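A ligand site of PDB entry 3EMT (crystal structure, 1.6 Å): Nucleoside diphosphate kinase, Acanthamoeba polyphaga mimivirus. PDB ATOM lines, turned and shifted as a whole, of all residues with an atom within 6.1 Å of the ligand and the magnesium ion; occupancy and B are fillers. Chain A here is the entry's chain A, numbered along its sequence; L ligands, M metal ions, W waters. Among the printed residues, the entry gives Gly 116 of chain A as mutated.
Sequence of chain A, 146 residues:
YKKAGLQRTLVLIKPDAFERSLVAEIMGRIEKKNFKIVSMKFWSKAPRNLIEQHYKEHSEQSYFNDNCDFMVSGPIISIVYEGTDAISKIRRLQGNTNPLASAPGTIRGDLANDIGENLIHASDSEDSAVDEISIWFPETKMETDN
The side-chain hydroxyl (OG1) of Thr 97 lies within hydrogen-bond range of an oxygen (O1) of the ligand (2.6 Å).
The guanidinium group (NH1) of Arg 91 is in salt-bridge range of an oxygen (O1) of the ligand.
The guanidinium group (NH1) of Arg 108 is in salt-bridge range of an oxygen (O1) of the ligand, 2.7 Å away.
An oxygen (O9) of the ligand lies within hydrogen-bond range of the side-chain amide nitrogen of Asn 118 (2.9 Å).
The side-chain amino group (NZ) of Lys 14 sits at hydrogen-bond distance from an oxygen (O9) of the ligand, at 3.0 Å.
A ring nitrogen (NE2) of His 58 lies close to an oxygen (O6) of the ligand (3.4 Å).
NE2 of Gln 94 lies close to NH1 of Arg 91, 3.1 Å away.
OD1 of Asn 118 sits at hydrogen-bond distance from NH2 of Arg 108, at 3.1 Å.
The backbone carbonyl oxygen (O) of Gln 94 lies within hydrogen-bond range of the backbone NH (N) of Arg 108 (2.9 Å).
The guanidinium group of Arg 108 lies within hydrogen-bond range of the backbone carbonyl oxygen of Gly 95 (3.1 Å).
ND2 of Asn 118 is in hydrogen-bond range of O of Ile 115, at 2.9 Å.
ND2 of Asn 118 lies within hydrogen-bond range of O of Gly 116 (3.5 Å).
The side-chain amino group of Lys 14 lies within hydrogen-bond range of the side-chain hydroxyl of Tyr 55.
ND1 of His 58 sits at hydrogen-bond distance from OH of Tyr 63, 2.7 Å away.
Residues that only touch the ligand: Tyr 63 (3.4 Å), Ile 115 (3.4 Å), Tyr 55 (3.6 Å) and Asn 67 (3.9 Å).
Hydrophobic or aromatic side chains within 4 Å of the ligand: Tyr 55, His 58, Tyr 63 and Ile 115.
Ten residues have an atom within 4 Å of the ligand: Lys 14, Tyr 55, His 58, Tyr 63, Asn 67, Arg 91, Thr 97, Arg 108, Ile 115 and Asn 118.
No residue comes within 4 Å of the magnesium ion.
The nearest printed residue that does not touch the magnesium ion is Arg 91 (4.1 Å).
The magnesium ion is bound by O6 of the ligand (2.2 Å), O2 of the ligand (2.2 Å) and water W7 (2.4 Å).
Slightly farther from the magnesium ion lies water W8 (2.7 Å).
Water W1 bridges O5 of the ligand (2.5 Å) and OG1 of Thr 97 (2.7 Å).
Water W4 bridges O5 of the ligand and OH of Tyr 63.
Water W9 lies within hydrogen-bond range of an oxygen (O3) of the ligand (2.6 Å), the side-chain hydroxyl (OH) of Tyr 55 (2.6 Å), a ring nitrogen (ND1) of His 121 (2.8 Å) and the side-chain amino group (NZ) of Lys 14 (3.1 Å).
Water W2 lies within hydrogen-bond range of N3 of the ligand (2.7 Å) and OD1 of Asn 67 (3.4 Å).
Water W5 lies within hydrogen-bond range of an oxygen (O1) of the ligand (2.7 Å) and the side-chain hydroxyl of Thr 97 (3.1 Å).
Water W6 lies within hydrogen-bond range of the side-chain amide oxygen of Gln 94 (2.9 Å), the backbone NH of Ala 122 (2.9 Å), an oxygen (O3) of the ligand (3.1 Å), the guanidinium group of Arg 91 (3.2 Å) and a ring nitrogen (ND1) of His 121 (3.2 Å).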
ATOM      1  N   LYS A  14      -5.090  27.343  19.920  1.00  0.00           N
ATOM      2  CA  LYS A  14      -4.199  26.190  19.839  1.00  0.00           C
ATOM      3  C   LYS A  14      -4.928  24.885  19.456  1.00  0.00           C
ATOM      4  O   LYS A  14      -6.154  24.815  19.482  1.00  0.00           O
ATOM      5  CB  LYS A  14      -3.449  26.036  21.172  1.00  0.00           C
ATOM      6  CG  LYS A  14      -2.545  27.217  21.488  1.00  0.00           C
ATOM      7  CD  LYS A  14      -1.769  26.984  22.786  1.00  0.00           C
ATOM      8  CE  LYS A  14      -0.729  28.073  23.062  1.00  0.00           C
ATOM      9  NZ  LYS A  14       0.034  27.768  24.333  1.00  0.00           N
ATOM     10  N   TYR A  55       8.225  30.372  19.649  1.00  0.00           N
ATOM     11  CA  TYR A  55       8.646  30.011  21.007  1.00  0.00           C
ATOM     12  C   TYR A  55      10.167  29.963  21.172  1.00  0.00           C
ATOM     13  O   TYR A  55      10.686  29.228  22.018  1.00  0.00           O
ATOM     14  CB  TYR A  55       8.051  28.656  21.393  1.00  0.00           C
ATOM     15  CG  TYR A  55       6.565  28.708  21.718  1.00  0.00           C
ATOM     16  CD1 TYR A  55       5.657  27.919  21.024  1.00  0.00           C
ATOM     17  CD2 TYR A  55       6.088  29.552  22.702  1.00  0.00           C
ATOM     18  CE1 TYR A  55       4.294  27.962  21.329  1.00  0.00           C
ATOM     19  CE2 TYR A  55       4.728  29.607  23.013  1.00  0.00           C
ATOM     20  CZ  TYR A  55       3.847  28.808  22.326  1.00  0.00           C
ATOM     21  OH  TYR A  55       2.497  28.855  22.630  1.00  0.00           O
ATOM     22  N   HIS A  58      12.047  29.770  24.476  1.00  0.00           N
ATOM     23  CA  HIS A  58      11.928  28.532  25.252  1.00  0.00           C
ATOM     24  C   HIS A  58      12.791  27.401  24.707  1.00  0.00           C
ATOM     25  O   HIS A  58      12.663  26.245  25.126  1.00  0.00           O
ATOM     26  CB  HIS A  58      10.466  28.072  25.276  1.00  0.00           C
ATOM     27  CG  HIS A  58       9.533  29.076  25.881  1.00  0.00           C
ATOM     28  ND1 HIS A  58       9.022  28.947  27.153  1.00  0.00           N
ATOM     29  CD2 HIS A  58       9.014  30.229  25.388  1.00  0.00           C
ATOM     30  CE1 HIS A  58       8.250  29.969  27.421  1.00  0.00           C
ATOM     31  NE2 HIS A  58       8.213  30.758  26.367  1.00  0.00           N
ATOM     32  N   TYR A  63      10.636  21.292  27.888  1.00  0.00           N
ATOM     33  CA  TYR A  63       9.363  21.053  27.209  1.00  0.00           C
ATOM     34  C   TYR A  63       9.337  21.577  25.778  1.00  0.00           C
ATOM     35  O   TYR A  63       8.320  21.445  25.109  1.00  0.00           O
ATOM     36  CB  TYR A  63       8.203  21.686  27.980  1.00  0.00           C
ATOM     37  CG  TYR A  63       8.429  23.150  28.299  1.00  0.00           C
ATOM     38  CD1 TYR A  63       8.205  24.125  27.341  1.00  0.00           C
ATOM     39  CD2 TYR A  63       8.879  23.552  29.557  1.00  0.00           C
ATOM     40  CE1 TYR A  63       8.427  25.466  27.616  1.00  0.00           C
ATOM     41  CE2 TYR A  63       9.101  24.872  29.842  1.00  0.00           C
ATOM     42  CZ  TYR A  63       8.867  25.832  28.872  1.00  0.00           C
ATOM     43  OH  TYR A  63       9.082  27.149  29.150  1.00  0.00           O
ATOM     44  N   ASN A  67       6.288  20.742  23.272  1.00  0.00           N
ATOM     45  CA  ASN A  67       5.378  21.853  22.974  1.00  0.00           C
ATOM     46  C   ASN A  67       5.259  22.099  21.471  1.00  0.00           C
ATOM     47  O   ASN A  67       4.165  22.340  20.965  1.00  0.00           O
ATOM     48  CB  ASN A  67       5.811  23.120  23.696  1.00  0.00           C
ATOM     49  CG  ASN A  67       4.770  24.214  23.627  1.00  0.00           C
ATOM     50  OD1 ASN A  67       3.608  24.004  23.979  1.00  0.00           O
ATOM     51  ND2 ASN A  67       5.176  25.385  23.165  1.00  0.00           N
ATOM     52  N   ARG A  91      -4.321  39.347  27.903  1.00  0.00           N
ATOM     53  CA  ARG A  91      -3.530  38.504  28.804  1.00  0.00           C
ATOM     54  C   ARG A  91      -4.323  38.195  30.081  1.00  0.00           C
ATOM     55  O   ARG A  91      -4.311  37.066  30.568  1.00  0.00           O
ATOM     56  CB  ARG A  91      -2.199  39.184  29.154  1.00  0.00           C
ATOM     57  CG  ARG A  91      -1.173  39.079  28.032  1.00  0.00           C
ATOM     58  CD  ARG A  91      -0.557  37.684  27.948  1.00  0.00           C
ATOM     59  NE  ARG A  91       0.510  37.509  28.933  1.00  0.00           N
ATOM     60  CZ  ARG A  91       1.176  36.369  29.090  1.00  0.00           C
ATOM     61  NH1 ARG A  91       0.858  35.304  28.361  1.00  0.00           N
ATOM     62  NH2 ARG A  91       2.151  36.281  29.991  1.00  0.00           N
ATOM     63  N   GLN A  94      -6.973  35.707  29.305  1.00  0.00           N
ATOM     64  CA  GLN A  94      -6.358  34.412  29.033  1.00  0.00           C
ATOM     65  C   GLN A  94      -6.179  33.599  30.303  1.00  0.00           C
ATOM     66  O   GLN A  94      -6.530  32.423  30.364  1.00  0.00           O
ATOM     67  CB  GLN A  94      -4.985  34.629  28.370  1.00  0.00           C
ATOM     68  CG  GLN A  94      -4.138  33.365  28.190  1.00  0.00           C
ATOM     69  CD  GLN A  94      -2.748  33.685  27.644  1.00  0.00           C
ATOM     70  OE1 GLN A  94      -2.204  32.945  26.815  1.00  0.00           O
ATOM     71  NE2 GLN A  94      -2.183  34.775  28.108  1.00  0.00           N
ATOM     72  N   GLY A  95      -5.572  34.229  31.307  1.00  0.00           N
ATOM     73  CA  GLY A  95      -5.299  33.546  32.565  1.00  0.00           C
ATOM     74  C   GLY A  95      -3.914  32.933  32.614  1.00  0.00           C
ATOM     75  O   GLY A  95      -3.256  32.742  31.591  1.00  0.00           O
ATOM     76  N   ASN A  96      -3.484  32.616  33.831  1.00  0.00           N
ATOM     77  CA  ASN A  96      -2.146  32.107  34.034  1.00  0.00           C
ATOM     78  C   ASN A  96      -1.879  30.771  33.335  1.00  0.00           C
ATOM     79  O   ASN A  96      -2.789  29.954  33.171  1.00  0.00           O
ATOM     80  CB  ASN A  96      -1.871  31.993  35.536  1.00  0.00           C
ATOM     81  CG  ASN A  96      -0.392  31.867  35.833  1.00  0.00           C
ATOM     82  OD1 ASN A  96       0.099  30.763  36.051  1.00  0.00           O
ATOM     83  ND2 ASN A  96       0.314  32.986  35.802  1.00  0.00           N
ATOM     84  N   THR A  97      -0.629  30.557  32.912  1.00  0.00           N
ATOM     85  CA  THR A  97      -0.235  29.286  32.292  1.00  0.00           C
ATOM     86  C   THR A  97      -0.495  28.095  33.212  1.00  0.00           C
ATOM     87  O   THR A  97      -0.869  27.023  32.751  1.00  0.00           O
ATOM     88  CB  THR A  97       1.288  29.261  31.991  1.00  0.00           C
ATOM     89  OG1 THR A  97       1.779  30.593  31.777  1.00  0.00           O
ATOM     90  CG2 THR A  97       1.584  28.382  30.784  1.00  0.00           C
ATOM     91  N   ARG A 108      -8.360  30.157  30.535  1.00  0.00           N
ATOM     92  CA  ARG A 108      -7.659  28.987  31.042  1.00  0.00           C
ATOM     93  C   ARG A 108      -8.230  28.520  32.375  1.00  0.00           C
ATOM     94  O   ARG A 108      -8.323  27.330  32.632  1.00  0.00           O
ATOM     95  CB  ARG A 108      -6.167  29.279  31.177  1.00  0.00           C
ATOM     96  CG  ARG A 108      -5.473  29.361  29.823  1.00  0.00           C
ATOM     97  CD  ARG A 108      -4.090  29.936  29.983  1.00  0.00           C
ATOM     98  NE  ARG A 108      -3.274  29.766  28.779  1.00  0.00           N
ATOM     99  CZ  ARG A 108      -2.033  30.234  28.694  1.00  0.00           C
ATOM    100  NH1 ARG A 108      -1.542  30.940  29.710  1.00  0.00           N
ATOM    101  NH2 ARG A 108      -1.312  30.018  27.599  1.00  0.00           N
ATOM    102  N   ASP A 114      -4.238  21.779  31.852  1.00  0.00           N
ATOM    103  CA  ASP A 114      -2.868  21.350  31.638  1.00  0.00           C
ATOM    104  C   ASP A 114      -1.974  22.562  31.389  1.00  0.00           C
ATOM    105  O   ASP A 114      -2.399  23.562  30.823  1.00  0.00           O
ATOM    106  CB  ASP A 114      -2.784  20.394  30.450  1.00  0.00           C
ATOM    107  CG  ASP A 114      -1.404  19.801  30.276  1.00  0.00           C
ATOM    108  OD1 ASP A 114      -0.725  20.136  29.279  1.00  0.00           O
ATOM    109  OD2 ASP A 114      -0.973  19.026  31.159  1.00  0.00           O
ATOM    110  N   ILE A 115      -0.725  22.459  31.830  1.00  0.00           N
ATOM    111  CA  ILE A 115       0.234  23.553  31.661  1.00  0.00           C
ATOM    112  C   ILE A 115       0.614  23.764  30.194  1.00  0.00           C
ATOM    113  O   ILE A 115       0.900  24.883  29.779  1.00  0.00           O
ATOM    114  CB  ILE A 115       1.505  23.279  32.490  1.00  0.00           C
ATOM    115  CG1 ILE A 115       2.478  24.461  32.404  1.00  0.00           C
ATOM    116  CG2 ILE A 115       2.185  21.992  32.035  1.00  0.00           C
ATOM    117  CD1 ILE A 115       2.252  25.522  33.445  1.00  0.00           C
ATOM    118  N   GLY A 116       0.637  22.683  29.415  1.00  0.00           N
ATOM    119  CA  GLY A 116       1.012  22.759  28.006  1.00  0.00           C
ATOM    120  C   GLY A 116      -0.172  22.916  27.079  1.00  0.00           C
ATOM    121  O   GLY A 116      -0.196  23.805  26.227  1.00  0.00           O
ATOM    122  N   GLU A 117      -1.149  22.028  27.226  1.00  0.00           N
ATOM    123  CA  GLU A 117      -2.365  22.079  26.433  1.00  0.00           C
ATOM    124  C   GLU A 117      -3.285  23.103  27.092  1.00  0.00           C
ATOM    125  O   GLU A 117      -4.123  22.769  27.919  1.00  0.00           O
ATOM    126  CB  GLU A 117      -2.985  20.690  26.318  1.00  0.00           C
ATOM    127  CG  GLU A 117      -2.000  19.711  25.643  1.00  0.00           C
ATOM    128  CD  GLU A 117      -2.604  18.378  25.265  1.00  0.00           C
ATOM    129  OE1 GLU A 117      -1.854  17.538  24.729  1.00  0.00           O
ATOM    130  OE2 GLU A 117      -3.805  18.164  25.491  1.00  0.00           O
ATOM    131  N   ASN A 118      -3.092  24.363  26.723  1.00  0.00           N
ATOM    132  CA  ASN A 118      -3.690  25.462  27.479  1.00  0.00           C
ATOM    133  C   ASN A 118      -4.462  26.442  26.583  1.00  0.00           C
ATOM    134  O   ASN A 118      -4.644  27.607  26.948  1.00  0.00           O
ATOM    135  CB  ASN A 118      -2.624  26.164  28.325  1.00  0.00           C
ATOM    136  CG  ASN A 118      -1.530  26.786  27.482  1.00  0.00           C
ATOM    137  OD1 ASN A 118      -1.776  27.222  26.349  1.00  0.00           O
ATOM    138  ND2 ASN A 118      -0.308  26.798  28.004  1.00  0.00           N
ATOM    139  N   ILE A 120      -4.812  28.670  24.375  1.00  0.00           N
ATOM    140  CA  ILE A 120      -4.646  29.999  23.814  1.00  0.00           C
ATOM    141  C   ILE A 120      -3.296  30.617  24.113  1.00  0.00           C
ATOM    142  O   ILE A 120      -2.787  30.513  25.232  1.00  0.00           O
ATOM    143  CB  ILE A 120      -5.784  30.957  24.306  1.00  0.00           C
ATOM    144  CG1 ILE A 120      -5.552  32.392  23.809  1.00  0.00           C
ATOM    145  CG2 ILE A 120      -5.902  30.935  25.832  1.00  0.00           C
ATOM    146  CD1 ILE A 120      -6.747  33.336  24.028  1.00  0.00           C
ATOM    147  N   HIS A 121      -2.708  31.236  23.090  1.00  0.00           N
ATOM    148  CA  HIS A 121      -1.566  32.116  23.235  1.00  0.00           C
ATOM    149  C   HIS A 121      -2.010  33.568  23.118  1.00  0.00           C
ATOM    150  O   HIS A 121      -2.880  33.886  22.301  1.00  0.00           O
ATOM    151  CB  HIS A 121      -0.541  31.874  22.135  1.00  0.00           C
ATOM    152  CG  HIS A 121       0.540  32.899  22.118  1.00  0.00           C
ATOM    153  ND1 HIS A 121       1.676  32.794  22.885  1.00  0.00           N
ATOM    154  CD2 HIS A 121       0.634  34.097  21.483  1.00  0.00           C
ATOM    155  CE1 HIS A 121       2.436  33.856  22.716  1.00  0.00           C
ATOM    156  NE2 HIS A 121       1.828  34.665  21.866  1.00  0.00           N
ATOM    157  N   ALA A 122      -1.403  34.457  23.902  1.00  0.00           N
ATOM    158  CA  ALA A 122      -1.589  35.893  23.731  1.00  0.00           C
ATOM    159  C   ALA A 122      -0.267  36.613  23.964  1.00  0.00           C
ATOM    160  O   ALA A 122       0.443  36.290  24.911  1.00  0.00           O
ATOM    161  CB  ALA A 122      -2.654  36.398  24.698  1.00  0.00           C
ATOM    162  N   ASP A 124       2.654  38.937  25.229  1.00  0.00           N
ATOM    163  CA  ASP A 124       2.806  39.378  26.618  1.00  0.00           C
ATOM    164  C   ASP A 124       3.308  40.813  26.777  1.00  0.00           C
ATOM    165  O   ASP A 124       3.305  41.342  27.887  1.00  0.00           O
ATOM    166  CB  ASP A 124       3.696  38.402  27.415  1.00  0.00           C
ATOM    167  CG  ASP A 124       5.148  38.410  26.958  1.00  0.00           C
ATOM    168  OD1 ASP A 124       5.516  39.242  26.114  1.00  0.00           O
ATOM    169  OD2 ASP A 124       5.925  37.569  27.468  1.00  0.00           O
ATOM    170  N   GLU A 132       5.690  38.676  17.115  1.00  0.00           N
ATOM    171  CA  GLU A 132       4.773  37.575  16.805  1.00  0.00           C
ATOM    172  C   GLU A 132       3.864  37.887  15.612  1.00  0.00           C
ATOM    173  O   GLU A 132       3.611  37.029  14.772  1.00  0.00           O
ATOM    174  CB  GLU A 132       3.956  37.201  18.048  1.00  0.00           C
ATOM    175  CG  GLU A 132       4.827  36.554  19.123  1.00  0.00           C
ATOM    176  CD  GLU A 132       4.170  36.521  20.505  1.00  0.00           C
ATOM    177  OE1 GLU A 132       2.970  36.853  20.614  1.00  0.00           O
ATOM    178  OE2 GLU A 132       4.865  36.142  21.481  1.00  0.00           O
HETATM  179  O1  LIG L   1       1.060  31.714  29.524  1.00  0.00           O
HETATM  180  P1  LIG L   1       2.088  31.625  28.328  1.00  0.00           P
HETATM  181  O2  LIG L   1       2.522  33.233  27.852  1.00  0.00           O
HETATM  182  O3  LIG L   1       1.408  30.704  27.018  1.00  0.00           O
HETATM  183  O4  LIG L   1       3.365  30.855  28.976  1.00  0.00           O
HETATM  184  P2  LIG L   1       4.959  30.895  28.629  1.00  0.00           P
HETATM  185  O5  LIG L   1       5.688  30.943  30.041  1.00  0.00           O
HETATM  186  O6  LIG L   1       5.434  32.209  27.584  1.00  0.00           O
HETATM  187  O7  LIG L   1       5.229  29.478  27.967  1.00  0.00           O
HETATM  188  C1  LIG L   1       4.943  29.297  26.577  1.00  0.00           C
HETATM  189  C2  LIG L   1       4.332  27.925  26.381  1.00  0.00           C
HETATM  190  O8  LIG L   1       5.254  26.878  26.743  1.00  0.00           O
HETATM  191  C3  LIG L   1       3.115  27.690  27.272  1.00  0.00           C
HETATM  192  O9  LIG L   1       1.895  28.133  26.679  1.00  0.00           O
HETATM  193  C4  LIG L   1       3.100  26.192  27.474  1.00  0.00           C
HETATM  194  C5  LIG L   1       4.570  25.814  27.407  1.00  0.00           C
HETATM  195  N1  LIG L   1       5.092  25.718  28.787  1.00  0.00           N
HETATM  196  C6  LIG L   1       5.500  26.734  29.552  1.00  0.00           C
HETATM  197  N2  LIG L   1       5.917  26.239  30.747  1.00  0.00           N
HETATM  198  C7  LIG L   1       5.767  24.903  30.703  1.00  0.00           C
HETATM  199  C8  LIG L   1       5.254  24.576  29.461  1.00  0.00           C
HETATM  200  N3  LIG L   1       4.995  23.304  29.144  1.00  0.00           N
HETATM  201  C9  LIG L   1       5.250  22.334  30.036  1.00  0.00           C
HETATM  202  N4  LIG L   1       4.987  21.047  29.699  1.00  0.00           N
HETATM  203  N5  LIG L   1       5.762  22.614  31.240  1.00  0.00           N
HETATM  204  C10 LIG L   1       6.029  23.873  31.601  1.00  0.00           C
HETATM  205  O10 LIG L   1       6.504  24.133  32.731  1.00  0.00           O
HETATM  206 MG    MG M   1       4.318  33.887  26.714  1.00  0.00          MG
HETATM  207  O   HOH W   1       4.432  31.045  32.193  1.00  0.00           O
HETATM  208  O   HOH W   2       4.706  22.231  26.691  1.00  0.00           O
HETATM  209  O   HOH W   3       7.771  27.368  32.924  1.00  0.00           O
HETATM  210  O   HOH W   4       7.879  29.811  30.719  1.00  0.00           O
HETATM  211  O   HOH W   5       0.512  33.421  31.556  1.00  0.00           O
HETATM  212  O   HOH W   6       0.528  33.374  25.834  1.00  0.00           O
HETATM  213  O   HOH W   7       3.003  35.576  25.603  1.00  0.00           O
HETATM  214  O   HOH W   8       5.852  32.937  24.698  1.00  0.00           O
HETATM  215  O   HOH W   9       1.570  30.497  24.454  1.00  0.00           O
